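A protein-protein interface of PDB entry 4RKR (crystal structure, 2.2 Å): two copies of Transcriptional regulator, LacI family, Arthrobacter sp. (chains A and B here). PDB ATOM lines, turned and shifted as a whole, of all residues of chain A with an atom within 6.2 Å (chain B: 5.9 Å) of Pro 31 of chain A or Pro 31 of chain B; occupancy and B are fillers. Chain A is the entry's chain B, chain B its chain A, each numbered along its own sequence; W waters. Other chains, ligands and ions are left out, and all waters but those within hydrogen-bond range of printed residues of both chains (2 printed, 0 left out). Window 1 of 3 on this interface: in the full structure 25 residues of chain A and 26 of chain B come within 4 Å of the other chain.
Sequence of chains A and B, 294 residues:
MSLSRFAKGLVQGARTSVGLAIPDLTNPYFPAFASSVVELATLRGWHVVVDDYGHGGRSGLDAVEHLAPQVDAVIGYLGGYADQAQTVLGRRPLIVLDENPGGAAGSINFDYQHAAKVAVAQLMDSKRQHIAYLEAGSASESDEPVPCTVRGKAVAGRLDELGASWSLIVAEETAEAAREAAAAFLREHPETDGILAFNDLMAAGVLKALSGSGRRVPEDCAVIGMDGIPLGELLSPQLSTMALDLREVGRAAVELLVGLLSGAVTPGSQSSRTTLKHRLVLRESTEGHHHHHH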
ATOM      1  N   ILE A  22       2.982 -16.736  -0.569  1.00  0.00           N
ATOM      2  CA  ILE A  22       3.350 -15.391  -1.009  1.00  0.00           C
ATOM      3  C   ILE A  22       2.120 -14.637  -1.479  1.00  0.00           C
ATOM      4  O   ILE A  22       1.212 -15.233  -2.051  1.00  0.00           O
ATOM      5  CB  ILE A  22       4.394 -15.400  -2.137  1.00  0.00           C
ATOM      6  CG1 ILE A  22       3.972 -16.335  -3.265  1.00  0.00           C
ATOM      7  CG2 ILE A  22       5.768 -15.828  -1.630  1.00  0.00           C
ATOM      8  CD1 ILE A  22       4.877 -16.228  -4.467  1.00  0.00           C
ATOM      9  N   ASP A  24       1.588 -12.312  -3.753  1.00  0.00           N
ATOM     10  CA  ASP A  24       1.371 -12.229  -5.196  1.00  0.00           C
ATOM     11  C   ASP A  24       2.601 -12.717  -5.993  1.00  0.00           C
ATOM     12  O   ASP A  24       3.667 -12.997  -5.440  1.00  0.00           O
ATOM     13  CB  ASP A  24       0.971 -10.807  -5.620  1.00  0.00           C
ATOM     14  CG  ASP A  24       2.095  -9.821  -5.472  1.00  0.00           C
ATOM     15  OD1 ASP A  24       3.132 -10.007  -6.135  1.00  0.00           O
ATOM     16  OD2 ASP A  24       1.954  -8.865  -4.688  1.00  0.00           O
ATOM     17  N   LEU A  25       2.418 -12.847  -7.297  1.00  0.00           N
ATOM     18  CA  LEU A  25       3.512 -13.127  -8.210  1.00  0.00           C
ATOM     19  C   LEU A  25       3.786 -11.938  -9.122  1.00  0.00           C
ATOM     20  O   LEU A  25       4.737 -11.959  -9.903  1.00  0.00           O
ATOM     21  CB  LEU A  25       3.172 -14.372  -9.037  1.00  0.00           C
ATOM     22  CG  LEU A  25       3.284 -15.679  -8.251  1.00  0.00           C
ATOM     23  CD1 LEU A  25       2.540 -16.819  -8.941  1.00  0.00           C
ATOM     24  CD2 LEU A  25       4.750 -16.035  -8.040  1.00  0.00           C
ATOM     25  N   THR A  26       2.968 -10.896  -9.007  1.00  0.00           N
ATOM     26  CA  THR A  26       3.039  -9.746  -9.908  1.00  0.00           C
ATOM     27  C   THR A  26       4.156  -8.786  -9.527  1.00  0.00           C
ATOM     28  O   THR A  26       4.775  -8.201 -10.412  1.00  0.00           O
ATOM     29  CB  THR A  26       1.694  -8.981  -9.959  1.00  0.00           C
ATOM     30  OG1 THR A  26       1.268  -8.657  -8.628  1.00  0.00           O
ATOM     31  CG2 THR A  26       0.618  -9.830 -10.662  1.00  0.00           C
ATOM     32  N   ASN A  27       4.385  -8.599  -8.225  1.00  0.00           N
ATOM     33  CA  ASN A  27       5.563  -7.885  -7.741  1.00  0.00           C
ATOM     34  C   ASN A  27       6.744  -8.834  -7.906  1.00  0.00           C
ATOM     35  O   ASN A  27       6.776  -9.887  -7.268  1.00  0.00           O
ATOM     36  CB  ASN A  27       5.412  -7.436  -6.276  1.00  0.00           C
ATOM     37  CG  ASN A  27       6.697  -6.828  -5.694  1.00  0.00           C
ATOM     38  OD1 ASN A  27       7.725  -6.785  -6.353  1.00  0.00           O
ATOM     39  ND2 ASN A  27       6.628  -6.359  -4.445  1.00  0.00           N
ATOM     40  N   PRO A  28       7.721  -8.461  -8.755  1.00  0.00           N
ATOM     41  CA  PRO A  28       8.855  -9.344  -9.079  1.00  0.00           C
ATOM     42  C   PRO A  28       9.739  -9.736  -7.903  1.00  0.00           C
ATOM     43  O   PRO A  28      10.494 -10.700  -8.013  1.00  0.00           O
ATOM     44  CB  PRO A  28       9.677  -8.526 -10.095  1.00  0.00           C
ATOM     45  CG  PRO A  28       8.742  -7.508 -10.641  1.00  0.00           C
ATOM     46  CD  PRO A  28       7.773  -7.198  -9.532  1.00  0.00           C
ATOM     47  N   TYR A  29       9.660  -9.021  -6.785  1.00  0.00           N
ATOM     48  CA  TYR A  29      10.358  -9.481  -5.582  1.00  0.00           C
ATOM     49  C   TYR A  29       9.986 -10.934  -5.232  1.00  0.00           C
ATOM     50  O   TYR A  29      10.864 -11.763  -4.950  1.00  0.00           O
ATOM     51  CB  TYR A  29      10.079  -8.560  -4.376  1.00  0.00           C
ATOM     52  CG  TYR A  29      10.628  -9.121  -3.086  1.00  0.00           C
ATOM     53  CD1 TYR A  29      11.990  -9.071  -2.815  1.00  0.00           C
ATOM     54  CD2 TYR A  29       9.793  -9.742  -2.156  1.00  0.00           C
ATOM     55  CE1 TYR A  29      12.503  -9.597  -1.640  1.00  0.00           C
ATOM     56  CE2 TYR A  29      10.298 -10.264  -0.986  1.00  0.00           C
ATOM     57  CZ  TYR A  29      11.649 -10.190  -0.737  1.00  0.00           C
ATOM     58  OH  TYR A  29      12.157 -10.711   0.423  1.00  0.00           O
ATOM     59  N   PHE A  30       8.689 -11.235  -5.263  1.00  0.00           N
ATOM     60  CA  PHE A  30       8.194 -12.508  -4.731  1.00  0.00           C
ATOM     61  C   PHE A  30       8.606 -13.736  -5.537  1.00  0.00           C
ATOM     62  O   PHE A  30       9.017 -14.722  -4.944  1.00  0.00           O
ATOM     63  CB  PHE A  30       6.673 -12.453  -4.501  1.00  0.00           C
ATOM     64  CG  PHE A  30       6.296 -11.519  -3.400  1.00  0.00           C
ATOM     65  CD1 PHE A  30       6.675 -11.796  -2.095  1.00  0.00           C
ATOM     66  CD2 PHE A  30       5.635 -10.325  -3.668  1.00  0.00           C
ATOM     67  CE1 PHE A  30       6.375 -10.921  -1.070  1.00  0.00           C
ATOM     68  CE2 PHE A  30       5.336  -9.447  -2.646  1.00  0.00           C
ATOM     69  CZ  PHE A  30       5.703  -9.744  -1.346  1.00  0.00           C
ATOM     70  N   PRO A  31       8.542 -13.672  -6.882  1.00  0.00           N
ATOM     71  CA  PRO A  31       9.092 -14.797  -7.637  1.00  0.00           C
ATOM     72  C   PRO A  31      10.595 -14.998  -7.416  1.00  0.00           C
ATOM     73  O   PRO A  31      11.078 -16.126  -7.464  1.00  0.00           O
ATOM     74  CB  PRO A  31       8.804 -14.447  -9.105  1.00  0.00           C
ATOM     75  CG  PRO A  31       8.138 -13.141  -9.113  1.00  0.00           C
ATOM     76  CD  PRO A  31       7.790 -12.735  -7.723  1.00  0.00           C
ATOM     77  N   ALA A  32      11.335 -13.922  -7.181  1.00  0.00           N
ATOM     78  CA  ALA A  32      12.762 -14.062  -6.905  1.00  0.00           C
ATOM     79  C   ALA A  32      12.962 -14.669  -5.518  1.00  0.00           C
ATOM     80  O   ALA A  32      13.772 -15.567  -5.334  1.00  0.00           O
ATOM     81  CB  ALA A  32      13.464 -12.726  -7.021  1.00  0.00           C
ATOM     82  N   PHE A  33      12.197 -14.192  -4.550  1.00  0.00           N
ATOM     83  CA  PHE A  33      12.208 -14.789  -3.225  1.00  0.00           C
ATOM     84  C   PHE A  33      11.854 -16.280  -3.290  1.00  0.00           C
ATOM     85  O   PHE A  33      12.535 -17.133  -2.732  1.00  0.00           O
ATOM     86  CB  PHE A  33      11.214 -14.056  -2.329  1.00  0.00           C
ATOM     87  CG  PHE A  33      10.966 -14.735  -1.016  1.00  0.00           C
ATOM     88  CD1 PHE A  33      11.966 -14.777  -0.042  1.00  0.00           C
ATOM     89  CD2 PHE A  33       9.720 -15.317  -0.732  1.00  0.00           C
ATOM     90  CE1 PHE A  33      11.741 -15.399   1.191  1.00  0.00           C
ATOM     91  CE2 PHE A  33       9.497 -15.946   0.483  1.00  0.00           C
ATOM     92  CZ  PHE A  33      10.509 -15.993   1.448  1.00  0.00           C
ATOM     93  N   ALA A  34      10.778 -16.592  -3.987  1.00  0.00           N
ATOM     94  CA  ALA A  34      10.341 -17.962  -4.083  1.00  0.00           C
ATOM     95  C   ALA A  34      11.427 -18.835  -4.698  1.00  0.00           C
ATOM     96  O   ALA A  34      11.734 -19.922  -4.200  1.00  0.00           O
ATOM     97  CB  ALA A  34       9.075 -18.040  -4.914  1.00  0.00           C
ATOM     98  N   SER A  35      11.995 -18.351  -5.793  1.00  0.00           N
ATOM     99  CA  SER A  35      12.926 -19.138  -6.571  1.00  0.00           C
ATOM    100  C   SER A  35      14.113 -19.509  -5.725  1.00  0.00           C
ATOM    101  O   SER A  35      14.606 -20.637  -5.785  1.00  0.00           O
ATOM    102  CB  SER A  35      13.391 -18.361  -7.794  1.00  0.00           C
ATOM    103  OG  SER A  35      14.169 -19.180  -8.628  1.00  0.00           O
ATOM    104  N   SER A  36      14.556 -18.556  -4.919  1.00  0.00           N
ATOM    105  CA  SER A  36      15.671 -18.773  -4.000  1.00  0.00           C
ATOM    106  C   SER A  36      15.330 -19.837  -2.955  1.00  0.00           C
ATOM    107  O   SER A  36      16.065 -20.816  -2.790  1.00  0.00           O
ATOM    108  CB  SER A  36      16.048 -17.457  -3.320  1.00  0.00           C
ATOM    109  OG  SER A  36      17.118 -17.650  -2.424  1.00  0.00           O
ATOM    110  N   ILE B  22       5.585 -25.041 -13.478  1.00  0.00           N
ATOM    111  CA  ILE B  22       6.364 -24.135 -14.342  1.00  0.00           C
ATOM    112  C   ILE B  22       7.860 -24.410 -14.204  1.00  0.00           C
ATOM    113  O   ILE B  22       8.333 -24.751 -13.125  1.00  0.00           O
ATOM    114  CB  ILE B  22       6.086 -22.654 -14.052  1.00  0.00           C
ATOM    115  CG1 ILE B  22       6.128 -22.398 -12.553  1.00  0.00           C
ATOM    116  CG2 ILE B  22       4.725 -22.265 -14.594  1.00  0.00           C
ATOM    117  CD1 ILE B  22       5.998 -20.946 -12.172  1.00  0.00           C
ATOM    118  N   ASP B  24      10.557 -22.451 -14.328  1.00  0.00           N
ATOM    119  CA  ASP B  24      11.330 -21.484 -13.545  1.00  0.00           C
ATOM    120  C   ASP B  24      10.443 -20.293 -13.163  1.00  0.00           C
ATOM    121  O   ASP B  24       9.373 -20.092 -13.724  1.00  0.00           O
ATOM    122  CB  ASP B  24      12.562 -20.967 -14.318  1.00  0.00           C
ATOM    123  CG  ASP B  24      12.193 -20.087 -15.523  1.00  0.00           C
ATOM    124  OD1 ASP B  24      11.571 -19.017 -15.341  1.00  0.00           O
ATOM    125  OD2 ASP B  24      12.551 -20.449 -16.662  1.00  0.00           O
ATOM    126  N   LEU B  25      10.917 -19.493 -12.224  1.00  0.00           N
ATOM    127  CA  LEU B  25      10.230 -18.277 -11.821  1.00  0.00           C
ATOM    128  C   LEU B  25      11.069 -17.047 -12.145  1.00  0.00           C
ATOM    129  O   LEU B  25      10.706 -15.931 -11.760  1.00  0.00           O
ATOM    130  CB  LEU B  25       9.932 -18.334 -10.316  1.00  0.00           C
ATOM    131  CG  LEU B  25       8.701 -19.157  -9.924  1.00  0.00           C
ATOM    132  CD1 LEU B  25       8.721 -19.482  -8.442  1.00  0.00           C
ATOM    133  CD2 LEU B  25       7.430 -18.411 -10.294  1.00  0.00           C
ATOM    134  N   THR B  26      12.171 -17.279 -12.865  1.00  0.00           N
ATOM    135  CA  THR B  26      13.165 -16.265 -13.201  1.00  0.00           C
ATOM    136  C   THR B  26      12.908 -15.600 -14.559  1.00  0.00           C
ATOM    137  O   THR B  26      13.255 -14.446 -14.733  1.00  0.00           O
ATOM    138  CB  THR B  26      14.592 -16.862 -13.165  1.00  0.00           C
ATOM    139  OG1 THR B  26      14.635 -18.102 -13.890  1.00  0.00           O
ATOM    140  CG2 THR B  26      15.005 -17.124 -11.725  1.00  0.00           C
ATOM    141  N   ASN B  27      12.322 -16.320 -15.518  1.00  0.00           N
ATOM    142  CA  ASN B  27      11.849 -15.700 -16.775  1.00  0.00           C
ATOM    143  C   ASN B  27      10.481 -15.084 -16.486  1.00  0.00           C
ATOM    144  O   ASN B  27       9.537 -15.825 -16.269  1.00  0.00           O
ATOM    145  CB  ASN B  27      11.762 -16.744 -17.892  1.00  0.00           C
ATOM    146  CG  ASN B  27      11.070 -16.227 -19.156  1.00  0.00           C
ATOM    147  OD1 ASN B  27      10.673 -15.069 -19.252  1.00  0.00           O
ATOM    148  ND2 ASN B  27      10.940 -17.100 -20.139  1.00  0.00           N
ATOM    149  N   PRO B  28      10.370 -13.727 -16.465  1.00  0.00           N
ATOM    150  CA  PRO B  28       9.135 -13.040 -16.043  1.00  0.00           C
ATOM    151  C   PRO B  28       7.855 -13.532 -16.689  1.00  0.00           C
ATOM    152  O   PRO B  28       6.779 -13.307 -16.133  1.00  0.00           O
ATOM    153  CB  PRO B  28       9.377 -11.588 -16.458  1.00  0.00           C
ATOM    154  CG  PRO B  28      10.845 -11.435 -16.367  1.00  0.00           C
ATOM    155  CD  PRO B  28      11.423 -12.755 -16.799  1.00  0.00           C
ATOM    156  N   TYR B  29       7.959 -14.189 -17.846  1.00  0.00           N
ATOM    157  CA  TYR B  29       6.787 -14.794 -18.461  1.00  0.00           C
ATOM    158  C   TYR B  29       6.045 -15.726 -17.507  1.00  0.00           C
ATOM    159  O   TYR B  29       4.823 -15.675 -17.410  1.00  0.00           O
ATOM    160  CB  TYR B  29       7.150 -15.559 -19.740  1.00  0.00           C
ATOM    161  CG  TYR B  29       5.964 -16.301 -20.301  1.00  0.00           C
ATOM    162  CD1 TYR B  29       4.981 -15.630 -21.030  1.00  0.00           C
ATOM    163  CD2 TYR B  29       5.787 -17.669 -20.054  1.00  0.00           C
ATOM    164  CE1 TYR B  29       3.863 -16.302 -21.522  1.00  0.00           C
ATOM    165  CE2 TYR B  29       4.675 -18.347 -20.535  1.00  0.00           C
ATOM    166  CZ  TYR B  29       3.718 -17.662 -21.269  1.00  0.00           C
ATOM    167  OH  TYR B  29       2.619 -18.331 -21.755  1.00  0.00           O
ATOM    168  N   PHE B  30       6.770 -16.584 -16.807  1.00  0.00           N
ATOM    169  CA  PHE B  30       6.090 -17.624 -16.032  1.00  0.00           C
ATOM    170  C   PHE B  30       5.356 -17.113 -14.808  1.00  0.00           C
ATOM    171  O   PHE B  30       4.242 -17.539 -14.549  1.00  0.00           O
ATOM    172  CB  PHE B  30       7.038 -18.759 -15.693  1.00  0.00           C
ATOM    173  CG  PHE B  30       7.516 -19.498 -16.908  1.00  0.00           C
ATOM    174  CD1 PHE B  30       6.629 -20.257 -17.662  1.00  0.00           C
ATOM    175  CD2 PHE B  30       8.834 -19.404 -17.320  1.00  0.00           C
ATOM    176  CE1 PHE B  30       7.058 -20.923 -18.787  1.00  0.00           C
ATOM    177  CE2 PHE B  30       9.273 -20.077 -18.440  1.00  0.00           C
ATOM    178  CZ  PHE B  30       8.381 -20.836 -19.178  1.00  0.00           C
ATOM    179  N   PRO B  31       5.952 -16.180 -14.060  1.00  0.00           N
ATOM    180  CA  PRO B  31       5.149 -15.638 -12.963  1.00  0.00           C
ATOM    181  C   PRO B  31       3.859 -15.002 -13.470  1.00  0.00           C
ATOM    182  O   PRO B  31       2.811 -15.167 -12.856  1.00  0.00           O
ATOM    183  CB  PRO B  31       6.062 -14.585 -12.311  1.00  0.00           C
ATOM    184  CG  PRO B  31       7.429 -14.824 -12.841  1.00  0.00           C
ATOM    185  CD  PRO B  31       7.379 -15.839 -13.948  1.00  0.00           C
ATOM    186  N   ALA B  32       3.937 -14.303 -14.600  1.00  0.00           N
ATOM    187  CA  ALA B  32       2.748 -13.675 -15.193  1.00  0.00           C
ATOM    188  C   ALA B  32       1.731 -14.720 -15.607  1.00  0.00           C
ATOM    189  O   ALA B  32       0.538 -14.554 -15.371  1.00  0.00           O
ATOM    190  CB  ALA B  32       3.130 -12.804 -16.380  1.00  0.00           C
ATOM    191  N   PHE B  33       2.218 -15.800 -16.218  1.00  0.00           N
ATOM    192  CA  PHE B  33       1.372 -16.921 -16.613  1.00  0.00           C
ATOM    193  C   PHE B  33       0.715 -17.553 -15.393  1.00  0.00           C
ATOM    194  O   PHE B  33      -0.497 -17.742 -15.355  1.00  0.00           O
ATOM    195  CB  PHE B  33       2.207 -17.962 -17.363  1.00  0.00           C
ATOM    196  CG  PHE B  33       1.520 -19.275 -17.547  1.00  0.00           C
ATOM    197  CD1 PHE B  33       0.457 -19.396 -18.427  1.00  0.00           C
ATOM    198  CD2 PHE B  33       1.941 -20.391 -16.854  1.00  0.00           C
ATOM    199  CE1 PHE B  33      -0.175 -20.610 -18.613  1.00  0.00           C
ATOM    200  CE2 PHE B  33       1.309 -21.603 -17.031  1.00  0.00           C
ATOM    201  CZ  PHE B  33       0.251 -21.714 -17.913  1.00  0.00           C
ATOM    202  N   ALA B  34       1.527 -17.855 -14.397  1.00  0.00           N
ATOM    203  CA  ALA B  34       1.061 -18.499 -13.185  1.00  0.00           C
ATOM    204  C   ALA B  34       0.006 -17.675 -12.494  1.00  0.00           C
ATOM    205  O   ALA B  34      -1.057 -18.203 -12.158  1.00  0.00           O
ATOM    206  CB  ALA B  34       2.222 -18.735 -12.235  1.00  0.00           C
ATOM    207  N   SER B  35       0.297 -16.388 -12.287  1.00  0.00           N
ATOM    208  CA  SER B  35      -0.637 -15.476 -11.605  1.00  0.00           C
ATOM    209  C   SER B  35      -2.011 -15.507 -12.277  1.00  0.00           C
ATOM    210  O   SER B  35      -3.053 -15.507 -11.635  1.00  0.00           O
ATOM    211  CB  SER B  35      -0.088 -14.049 -11.628  1.00  0.00           C
ATOM    212  OG  SER B  35      -0.877 -13.166 -10.851  1.00  0.00           O
ATOM    213  N   SER B  36      -1.998 -15.528 -13.595  1.00  0.00           N
ATOM    214  CA  SER B  36      -3.218 -15.438 -14.360  1.00  0.00           C
ATOM    215  C   SER B  36      -4.046 -16.671 -14.101  1.00  0.00           C
ATOM    216  O   SER B  36      -5.229 -16.581 -13.791  1.00  0.00           O
ATOM    217  CB  SER B  36      -2.880 -15.308 -15.851  1.00  0.00           C
ATOM    218  OG  SER B  36      -4.036 -15.418 -16.648  1.00  0.00           O
HETATM  219  O   HOH W   1      -0.204 -13.069  -8.319  1.00  0.00           O
HETATM  220  O   HOH W   2      12.915 -20.444 -10.575  1.00  0.00           O
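Of the printed residues of chain B, Pro 31 of chain A touches Leu 25 (3.6 Å) and Pro 31 (3.999 Å).
Printed residues of chain B within 4 Å of Ser 35 of chain A: Thr 26 (3.8 Å).
Of the printed residues of chain A, Thr 26 of chain B touches Ser 35.
Pro 28 of chain B touches none of the printed residues of chain A.
Printed residues of chain A within 4 Å of Pro 31 of chain B: Leu 25 (3.8 Å) and Pro 31 (3.999 Å).
Of the printed residues of chain A, Ala 34 of chain B touches Leu 25 (3.8 Å).
Printed residues of chain A within 4 Å of Ser 35 of chain B: Thr 26.
The nearest printed residue of chain B that does not touch Thr 26 of chain A is Pro 31 of chain B (5.8 Å).
Water W1 bridges OG of Ser 35 of chain B and N of Leu 25 of chain A.
Water W2 lies within hydrogen-bond range of the side-chain hydroxyl (OG) of Ser 35 of chain A and the backbone NH (N) of Leu 25 of chain B.
Of the 14 printed residues of chain B, 5 touch a printed residue of chain A.
Printed residues of chain B that touch a printed residue of chain A: Leu 25, Thr 26, Pro 31, Ala 34 and Ser 35.
Hydrophobic or aromatic side chains of chain B that line the printed part of chain A: Leu 25, Pro 31 and Ala 34.
Hydrophobic or aromatic side chains of chain A that line the printed part of chain B: Leu 25, Pro 31 and Ala 34.
The backbone NH (N) of Thr 26 of chain A lies within hydrogen-bond range of the side-chain carboxylate (OD1) of Asp 24 of chain A, 3.0 Å away.
N of Thr 26 of chain B sits at hydrogen-bond distance from OD1 of Asp 24 of chain B (3.1 Å).
Among the printed residues, pairs that only touch across the chains: Leu 25 of chain A with Pro 31 of chain B, Leu 25 of chain A with Ala 34 of chain B, Thr 26 of chain A with Ser 35 of chain B, Pro 31 of chain A with Leu 25 of chain B, Pro 31 of chain A with Pro 31 of chain B, Ala 34 of chain A with Leu 25 of chain B and Ser 35 of chain A with Thr 26 of chain B.
Leu 25 of chain A touches Pro 31 of chain B, and with the chains exchanged Pro 31 of chain A touches Leu 25 of chain B.
Leu 25 of chain A touches Ala 34 of chain B, and with the chains exchanged Ala 34 of chain A touches Leu 25 of chain B.
Thr 26 of chain A touches Ser 35 of chain B, and with the chains exchanged Ser 35 of chain A touches Thr 26 of chain B.
Pro 31 of chain A touches its own counterpart, Pro 31 of chain B.
Positions printed for both chains: 22, 24, 25, 26, 27, 28, 29, 30, 31, 32, 33, 34, 35 and 36.
Of the 7 pairs that touch across the chains among the printed residues, 7 have their exchanged pair printed and touching as well.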
